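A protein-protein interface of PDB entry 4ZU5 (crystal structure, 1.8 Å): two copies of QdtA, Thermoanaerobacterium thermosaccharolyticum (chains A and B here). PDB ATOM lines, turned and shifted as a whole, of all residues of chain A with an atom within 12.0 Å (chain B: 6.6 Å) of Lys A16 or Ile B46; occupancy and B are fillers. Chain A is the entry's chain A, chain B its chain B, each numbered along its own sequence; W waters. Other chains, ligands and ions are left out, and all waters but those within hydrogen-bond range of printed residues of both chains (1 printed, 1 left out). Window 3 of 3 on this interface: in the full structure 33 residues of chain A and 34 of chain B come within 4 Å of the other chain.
The backbone carbonyl oxygen (O) of Tyr A17 sits at hydrogen-bond distance from the guanidinium group (NH2) of Arg B48 (2.9 Å).
The side-chain carboxylate of Asp A12 is in hydrogen-bond range of a ring nitrogen (ND1) of His A19 (2.9 Å).
The backbone NH (N) of Ile A13 sits at hydrogen-bond distance from the backbone carbonyl oxygen (O) of Leu A20, at 2.8 Å.
OD1 of Asp A15 lies within hydrogen-bond range of N of Tyr A17 (2.8 Å).
The side-chain amino group of Lys A16 is in hydrogen-bond range of the side-chain hydroxyl of Tyr A17 (2.8 Å).
The backbone carbonyl oxygen (O) of Arg B48 lies within hydrogen-bond range of the backbone NH (N) of Met B99 (2.7 Å).
OD1 of Asp A15 lies within hydrogen-bond range of N of Gly A18 (3.4 Å).
Among the printed residues, pairs that only touch across the chains: Lys A16 with Ile B46, Tyr A17 with Val B42, Tyr A17 with Ile B46, Tyr A17 with Thr B47, Gly A18 with Lys B41, Gly A18 with Arg B48, His A19 with Lys B41 and Leu A20 with Arg B48.
Ile B46 touches two residues of chain A.
Val B42 touches just one residue of chain A: Tyr A17 (3.5 Å).
No residue of chain A comes within 4 Å of Asp B43.
No residue of chain A comes within 4 Å of Asp B45.
Of chain A, only Tyr A17 comes within 4 Å of Thr B47.
Arg B48 touches just these residues of chain A: Tyr A17, Gly A18 and Leu A20.
No residue of chain A comes within 4 Å of Phe B102.
Printed residues of chain B within 4 Å of Gly A18: Lys B41 and Arg B48.
Printed residues of chain B within 4 Å of Leu A20: Arg B48 (3.6 Å).
Asp A15 touches none of the printed residues of chain B.
The nearest residue of chain A that does not touch Ile B46 is Gly A18 (5.6 Å).
Of the 12 printed residues of chain B, 5 touch a printed residue of chain A.
Hydrophobic or aromatic side chains of chain B within 4 Å of the printed part of chain A: Val B42 and Ile B46.
Of the 9 printed residues of chain A, 5 touch a printed residue of chain B.
Hydrophobic or aromatic side chains of chain A that line the printed part of chain B: Tyr A17, His A19 and Leu A20.
No position is printed for both chains.
Of the 9 pairs that touch across the chains among the printed residues, none has its exchanged pair printed and touching as well.
Water W1 lies within hydrogen-bond range of the backbone carbonyl oxygen (O) of Lys A16 (2.7 Å), the backbone NH (N) of Asp B43 (3.0 Å) and the backbone NH (N) of Gly A18 (3.2 Å).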
ATOM      1  N   ASP A  12      17.360 -11.808  10.767  1.00  0.00           N
ATOM      2  CA  ASP A  12      18.269 -10.655  10.669  1.00  0.00           C
ATOM      3  C   ASP A  12      19.395 -11.010   9.702  1.00  0.00           C
ATOM      4  O   ASP A  12      20.302 -11.741  10.073  1.00  0.00           O
ATOM      5  CB  ASP A  12      18.866 -10.355  12.038  1.00  0.00           C
ATOM      6  CG  ASP A  12      19.844  -9.194  12.006  1.00  0.00           C
ATOM      7  OD1 ASP A  12      19.929  -8.508  10.974  1.00  0.00           O
ATOM      8  OD2 ASP A  12      20.515  -8.962  13.024  1.00  0.00           O
ATOM      9  N   ILE A  13      19.306 -10.576   8.456  1.00  0.00           N
ATOM     10  CA  ILE A  13      20.344 -10.831   7.478  1.00  0.00           C
ATOM     11  C   ILE A  13      21.455  -9.803   7.669  1.00  0.00           C
ATOM     12  O   ILE A  13      21.286  -8.620   7.377  1.00  0.00           O
ATOM     13  CB  ILE A  13      19.740 -10.780   6.088  1.00  0.00           C
ATOM     14  CG1 ILE A  13      18.731 -11.926   5.969  1.00  0.00           C
ATOM     15  CG2 ILE A  13      20.816 -10.812   5.007  1.00  0.00           C
ATOM     16  CD1 ILE A  13      17.999 -11.939   4.657  1.00  0.00           C
ATOM     17  N   ALA A  14      22.559 -10.244   8.257  1.00  0.00           N
ATOM     18  CA  ALA A  14      23.672  -9.382   8.580  1.00  0.00           C
ATOM     19  C   ALA A  14      24.881  -9.808   7.740  1.00  0.00           C
ATOM     20  O   ALA A  14      25.249 -10.972   7.620  1.00  0.00           O
ATOM     21  CB  ALA A  14      23.963  -9.455  10.063  1.00  0.00           C
ATOM     22  N   ASP A  15      25.435  -8.866   7.011  1.00  0.00           N
ATOM     23  CA  ASP A  15      26.649  -9.175   6.269  1.00  0.00           C
ATOM     24  C   ASP A  15      27.359  -7.853   6.124  1.00  0.00           C
ATOM     25  O   ASP A  15      27.047  -6.903   6.824  1.00  0.00           O
ATOM     26  CB  ASP A  15      26.343  -9.789   4.901  1.00  0.00           C
ATOM     27  CG  ASP A  15      25.445  -8.916   4.057  1.00  0.00           C
ATOM     28  OD1 ASP A  15      25.257  -7.714   4.351  1.00  0.00           O
ATOM     29  OD2 ASP A  15      24.879  -9.456   3.103  1.00  0.00           O
ATOM     30  N   LYS A  16      28.315  -7.762   5.207  1.00  0.00           N
ATOM     31  CA  LYS A  16      29.104  -6.527   5.126  1.00  0.00           C
ATOM     32  C   LYS A  16      28.269  -5.354   4.621  1.00  0.00           C
ATOM     33  O   LYS A  16      28.675  -4.193   4.751  1.00  0.00           O
ATOM     34  CB  LYS A  16      30.363  -6.718   4.252  1.00  0.00           C
ATOM     35  CG  LYS A  16      30.174  -6.589   2.744  1.00  0.00           C
ATOM     36  CD  LYS A  16      31.414  -7.100   2.030  1.00  0.00           C
ATOM     37  CE  LYS A  16      31.054  -7.880   0.782  1.00  0.00           C
ATOM     38  NZ  LYS A  16      30.662  -6.910  -0.273  1.00  0.00           N
ATOM     39  N   TYR A  17      27.129  -5.665   4.002  1.00  0.00           N
ATOM     40  CA  TYR A  17      26.216  -4.643   3.506  1.00  0.00           C
ATOM     41  C   TYR A  17      25.265  -4.060   4.551  1.00  0.00           C
ATOM     42  O   TYR A  17      24.527  -3.129   4.227  1.00  0.00           O
ATOM     43  CB  TYR A  17      25.424  -5.171   2.307  1.00  0.00           C
ATOM     44  CG  TYR A  17      26.303  -5.507   1.128  1.00  0.00           C
ATOM     45  CD1 TYR A  17      26.878  -4.497   0.370  1.00  0.00           C
ATOM     46  CD2 TYR A  17      26.551  -6.833   0.769  1.00  0.00           C
ATOM     47  CE1 TYR A  17      27.671  -4.784  -0.722  1.00  0.00           C
ATOM     48  CE2 TYR A  17      27.356  -7.131  -0.311  1.00  0.00           C
ATOM     49  CZ  TYR A  17      27.908  -6.101  -1.052  1.00  0.00           C
ATOM     50  OH  TYR A  17      28.689  -6.362  -2.146  1.00  0.00           O
ATOM     51  N   GLY A  18      25.294  -4.594   5.775  1.00  0.00           N
ATOM     52  CA  GLY A  18      24.484  -4.098   6.882  1.00  0.00           C
ATOM     53  C   GLY A  18      23.516  -5.163   7.382  1.00  0.00           C
ATOM     54  O   GLY A  18      23.794  -6.352   7.284  1.00  0.00           O
ATOM     55  N   HIS A  19      22.371  -4.741   7.902  1.00  0.00           N
ATOM     56  CA  HIS A  19      21.362  -5.659   8.383  1.00  0.00           C
ATOM     57  C   HIS A  19      20.077  -5.415   7.627  1.00  0.00           C
ATOM     58  O   HIS A  19      19.706  -4.257   7.460  1.00  0.00           O
ATOM     59  CB  HIS A  19      21.085  -5.366   9.833  1.00  0.00           C
ATOM     60  CG  HIS A  19      22.233  -5.691  10.710  1.00  0.00           C
ATOM     61  ND1 HIS A  19      22.215  -6.770  11.565  1.00  0.00           N
ATOM     62  CD2 HIS A  19      23.484  -5.180  10.757  1.00  0.00           C
ATOM     63  CE1 HIS A  19      23.379  -6.843  12.184  1.00  0.00           C
ATOM     64  NE2 HIS A  19      24.167  -5.902  11.702  1.00  0.00           N
ATOM     65  N   LEU A  20      19.356  -6.501   7.341  1.00  0.00           N
ATOM     66  CA  LEU A  20      18.038  -6.441   6.756  1.00  0.00           C
ATOM     67  C   LEU A  20      17.155  -7.455   7.463  1.00  0.00           C
ATOM     68  O   LEU A  20      17.508  -8.646   7.584  1.00  0.00           O
ATOM     69  CB  LEU A  20      18.071  -6.802   5.283  1.00  0.00           C
ATOM     70  CG  LEU A  20      16.824  -6.630   4.417  1.00  0.00           C
ATOM     71  CD1 LEU A  20      17.155  -6.321   2.970  1.00  0.00           C
ATOM     72  CD2 LEU A  20      15.991  -7.914   4.462  1.00  0.00           C
ATOM     73  N   LYS B  41      21.959  -0.151  10.194  1.00  0.00           N
ATOM     74  CA  LYS B  41      23.347  -0.404  10.577  1.00  0.00           C
ATOM     75  C   LYS B  41      24.261  -0.555   9.379  1.00  0.00           C
ATOM     76  O   LYS B  41      25.141  -1.400   9.354  1.00  0.00           O
ATOM     77  CB  LYS B  41      23.414  -1.634  11.488  1.00  0.00           C
ATOM     78  CG  LYS B  41      22.793  -1.400  12.867  1.00  0.00           C
ATOM     79  CD  LYS B  41      22.834  -2.696  13.662  1.00  0.00           C
ATOM     80  CE  LYS B  41      21.523  -3.001  14.389  1.00  0.00           C
ATOM     81  NZ  LYS B  41      20.328  -3.239  13.508  1.00  0.00           N
ATOM     82  N   VAL B  42      24.000   0.191   8.309  1.00  0.00           N
ATOM     83  CA  VAL B  42      24.827   0.076   7.125  1.00  0.00           C
ATOM     84  C   VAL B  42      26.030   1.048   7.258  1.00  0.00           C
ATOM     85  O   VAL B  42      25.856   2.187   7.692  1.00  0.00           O
ATOM     86  CB  VAL B  42      24.025   0.467   5.861  1.00  0.00           C
ATOM     87  CG1 VAL B  42      24.930   0.449   4.655  1.00  0.00           C
ATOM     88  CG2 VAL B  42      22.823  -0.458   5.669  1.00  0.00           C
ATOM     89  N   ASP B  43      27.229   0.561   6.965  1.00  0.00           N
ATOM     90  CA  ASP B  43      28.433   1.387   7.125  1.00  0.00           C
ATOM     91  C   ASP B  43      28.468   2.457   6.061  1.00  0.00           C
ATOM     92  O   ASP B  43      27.920   2.231   4.994  1.00  0.00           O
ATOM     93  CB  ASP B  43      29.693   0.542   7.022  1.00  0.00           C
ATOM     94  CG  ASP B  43      29.862  -0.370   8.208  1.00  0.00           C
ATOM     95  OD1 ASP B  43      30.303  -1.511   7.984  1.00  0.00           O
ATOM     96  OD2 ASP B  43      29.530   0.028   9.341  1.00  0.00           O
ATOM     97  N   LYS B  44      29.162   3.572   6.337  1.00  0.00           N
ATOM     98  CA  LYS B  44      29.014   4.838   5.590  1.00  0.00           C
ATOM     99  C   LYS B  44      29.600   4.744   4.187  1.00  0.00           C
ATOM    100  O   LYS B  44      29.137   5.384   3.247  1.00  0.00           O
ATOM    101  CB  LYS B  44      29.597   6.026   6.358  1.00  0.00           C
ATOM    102  CG  LYS B  44      30.902   5.678   7.047  1.00  0.00           C
ATOM    103  CD  LYS B  44      31.585   6.852   7.735  1.00  0.00           C
ATOM    104  CE  LYS B  44      32.648   6.338   8.714  1.00  0.00           C
ATOM    105  NZ  LYS B  44      34.021   6.204   8.126  1.00  0.00           N
ATOM    106  N   ASP B  45      30.556   3.854   4.025  1.00  0.00           N
ATOM    107  CA  ASP B  45      31.226   3.693   2.739  1.00  0.00           C
ATOM    108  C   ASP B  45      30.520   2.654   1.847  1.00  0.00           C
ATOM    109  O   ASP B  45      30.990   2.382   0.733  1.00  0.00           O
ATOM    110  CB  ASP B  45      32.665   3.248   3.039  1.00  0.00           C
ATOM    111  CG  ASP B  45      32.703   1.956   3.888  1.00  0.00           C
ATOM    112  OD1 ASP B  45      31.830   1.755   4.778  1.00  0.00           O
ATOM    113  OD2 ASP B  45      33.591   1.104   3.663  1.00  0.00           O
ATOM    114  N   ILE B  46      29.427   2.039   2.336  1.00  0.00           N
ATOM    115  CA  ILE B  46      28.810   0.890   1.644  1.00  0.00           C
ATOM    116  C   ILE B  46      27.784   1.314   0.578  1.00  0.00           C
ATOM    117  O   ILE B  46      27.064   2.292   0.752  1.00  0.00           O
ATOM    118  CB  ILE B  46      28.087  -0.065   2.634  1.00  0.00           C
ATOM    119  CG1 ILE B  46      29.109  -0.821   3.487  1.00  0.00           C
ATOM    120  CG2 ILE B  46      27.180  -1.040   1.888  1.00  0.00           C
ATOM    121  CD1 ILE B  46      29.736  -2.029   2.815  1.00  0.00           C
ATOM    122  N   THR B  47      27.744   0.571  -0.514  1.00  0.00           N
ATOM    123  CA  THR B  47      26.673   0.689  -1.509  1.00  0.00           C
ATOM    124  C   THR B  47      26.033  -0.676  -1.572  1.00  0.00           C
ATOM    125  O   THR B  47      26.749  -1.682  -1.592  1.00  0.00           O
ATOM    126  CB  THR B  47      27.193   1.033  -2.908  1.00  0.00           C
ATOM    127  OG1 THR B  47      27.762   2.340  -2.898  1.00  0.00           O
ATOM    128  CG2 THR B  47      26.065   1.051  -3.919  1.00  0.00           C
ATOM    129  N   ARG B  48      24.687  -0.710  -1.535  1.00  0.00           N
ATOM    130  CA  ARG B  48      23.950  -1.970  -1.620  1.00  0.00           C
ATOM    131  C   ARG B  48      22.770  -1.880  -2.566  1.00  0.00           C
ATOM    132  O   ARG B  48      22.551  -0.866  -3.244  1.00  0.00           O
ATOM    133  CB  ARG B  48      23.485  -2.438  -0.228  1.00  0.00           C
ATOM    134  CG  ARG B  48      22.667  -1.465   0.605  1.00  0.00           C
ATOM    135  CD  ARG B  48      22.288  -2.105   1.941  1.00  0.00           C
ATOM    136  NE  ARG B  48      21.391  -3.247   1.716  1.00  0.00           N
ATOM    137  CZ  ARG B  48      21.319  -4.346   2.453  1.00  0.00           C
ATOM    138  NH1 ARG B  48      20.464  -5.282   2.109  1.00  0.00           N
ATOM    139  NH2 ARG B  48      22.080  -4.538   3.512  1.00  0.00           N
ATOM    140  N   MET B  99      21.800   1.732  -3.355  1.00  0.00           N
ATOM    141  CA  MET B  99      21.646   2.693  -2.299  1.00  0.00           C
ATOM    142  C   MET B  99      22.945   2.954  -1.566  1.00  0.00           C
ATOM    143  O   MET B  99      23.643   2.008  -1.249  1.00  0.00           O
ATOM    144  CB  MET B  99      20.661   2.155  -1.251  1.00  0.00           C
ATOM    145  CG  MET B  99      19.246   2.023  -1.770  1.00  0.00           C
ATOM    146  SD  MET B  99      18.932   0.358  -2.265  1.00  0.00           S
ATOM    147  CE  MET B  99      18.509  -0.208  -0.635  1.00  0.00           C
ATOM    148  N   PHE B 100      23.198   4.191  -1.186  1.00  0.00           N
ATOM    149  CA  PHE B 100      24.503   4.525  -0.598  1.00  0.00           C
ATOM    150  C   PHE B 100      24.397   5.736   0.259  1.00  0.00           C
ATOM    151  O   PHE B 100      23.340   6.347   0.370  1.00  0.00           O
ATOM    152  CB  PHE B 100      25.541   4.776  -1.702  1.00  0.00           C
ATOM    153  CG  PHE B 100      25.248   5.968  -2.575  1.00  0.00           C
ATOM    154  CD1 PHE B 100      25.940   7.163  -2.418  1.00  0.00           C
ATOM    155  CD2 PHE B 100      24.325   5.877  -3.601  1.00  0.00           C
ATOM    156  CE1 PHE B 100      25.681   8.250  -3.227  1.00  0.00           C
ATOM    157  CE2 PHE B 100      24.098   6.951  -4.443  1.00  0.00           C
ATOM    158  CZ  PHE B 100      24.753   8.146  -4.230  1.00  0.00           C
ATOM    159  N   ASP B 101      25.503   6.097   0.913  1.00  0.00           N
ATOM    160  CA  ASP B 101      25.488   7.176   1.871  1.00  0.00           C
ATOM    161  C   ASP B 101      24.434   7.012   2.950  1.00  0.00           C
ATOM    162  O   ASP B 101      23.683   7.945   3.269  1.00  0.00           O
ATOM    163  CB  ASP B 101      25.310   8.555   1.228  1.00  0.00           C
ATOM    164  CG  ASP B 101      26.603   9.064   0.523  1.00  0.00           C
ATOM    165  OD1 ASP B 101      27.592   8.310   0.504  1.00  0.00           O
ATOM    166  OD2 ASP B 101      26.568  10.167  -0.050  1.00  0.00           O
ATOM    167  N   PHE B 102      24.316   5.797   3.471  1.00  0.00           N
ATOM    168  CA  PHE B 102      23.512   5.605   4.641  1.00  0.00           C
ATOM    169  C   PHE B 102      24.172   6.311   5.808  1.00  0.00           C
ATOM    170  O   PHE B 102      25.324   6.036   6.126  1.00  0.00           O
ATOM    171  CB  PHE B 102      23.415   4.138   5.012  1.00  0.00           C
ATOM    172  CG  PHE B 102      22.516   3.333   4.110  1.00  0.00           C
ATOM    173  CD1 PHE B 102      22.966   2.890   2.896  1.00  0.00           C
ATOM    174  CD2 PHE B 102      21.294   2.890   4.572  1.00  0.00           C
ATOM    175  CE1 PHE B 102      22.185   2.081   2.086  1.00  0.00           C
ATOM    176  CE2 PHE B 102      20.504   2.066   3.780  1.00  0.00           C
ATOM    177  CZ  PHE B 102      20.941   1.670   2.527  1.00  0.00           C
HETATM  178  O   HOH W   1      27.529  -2.367   6.441  1.00  0.00           O
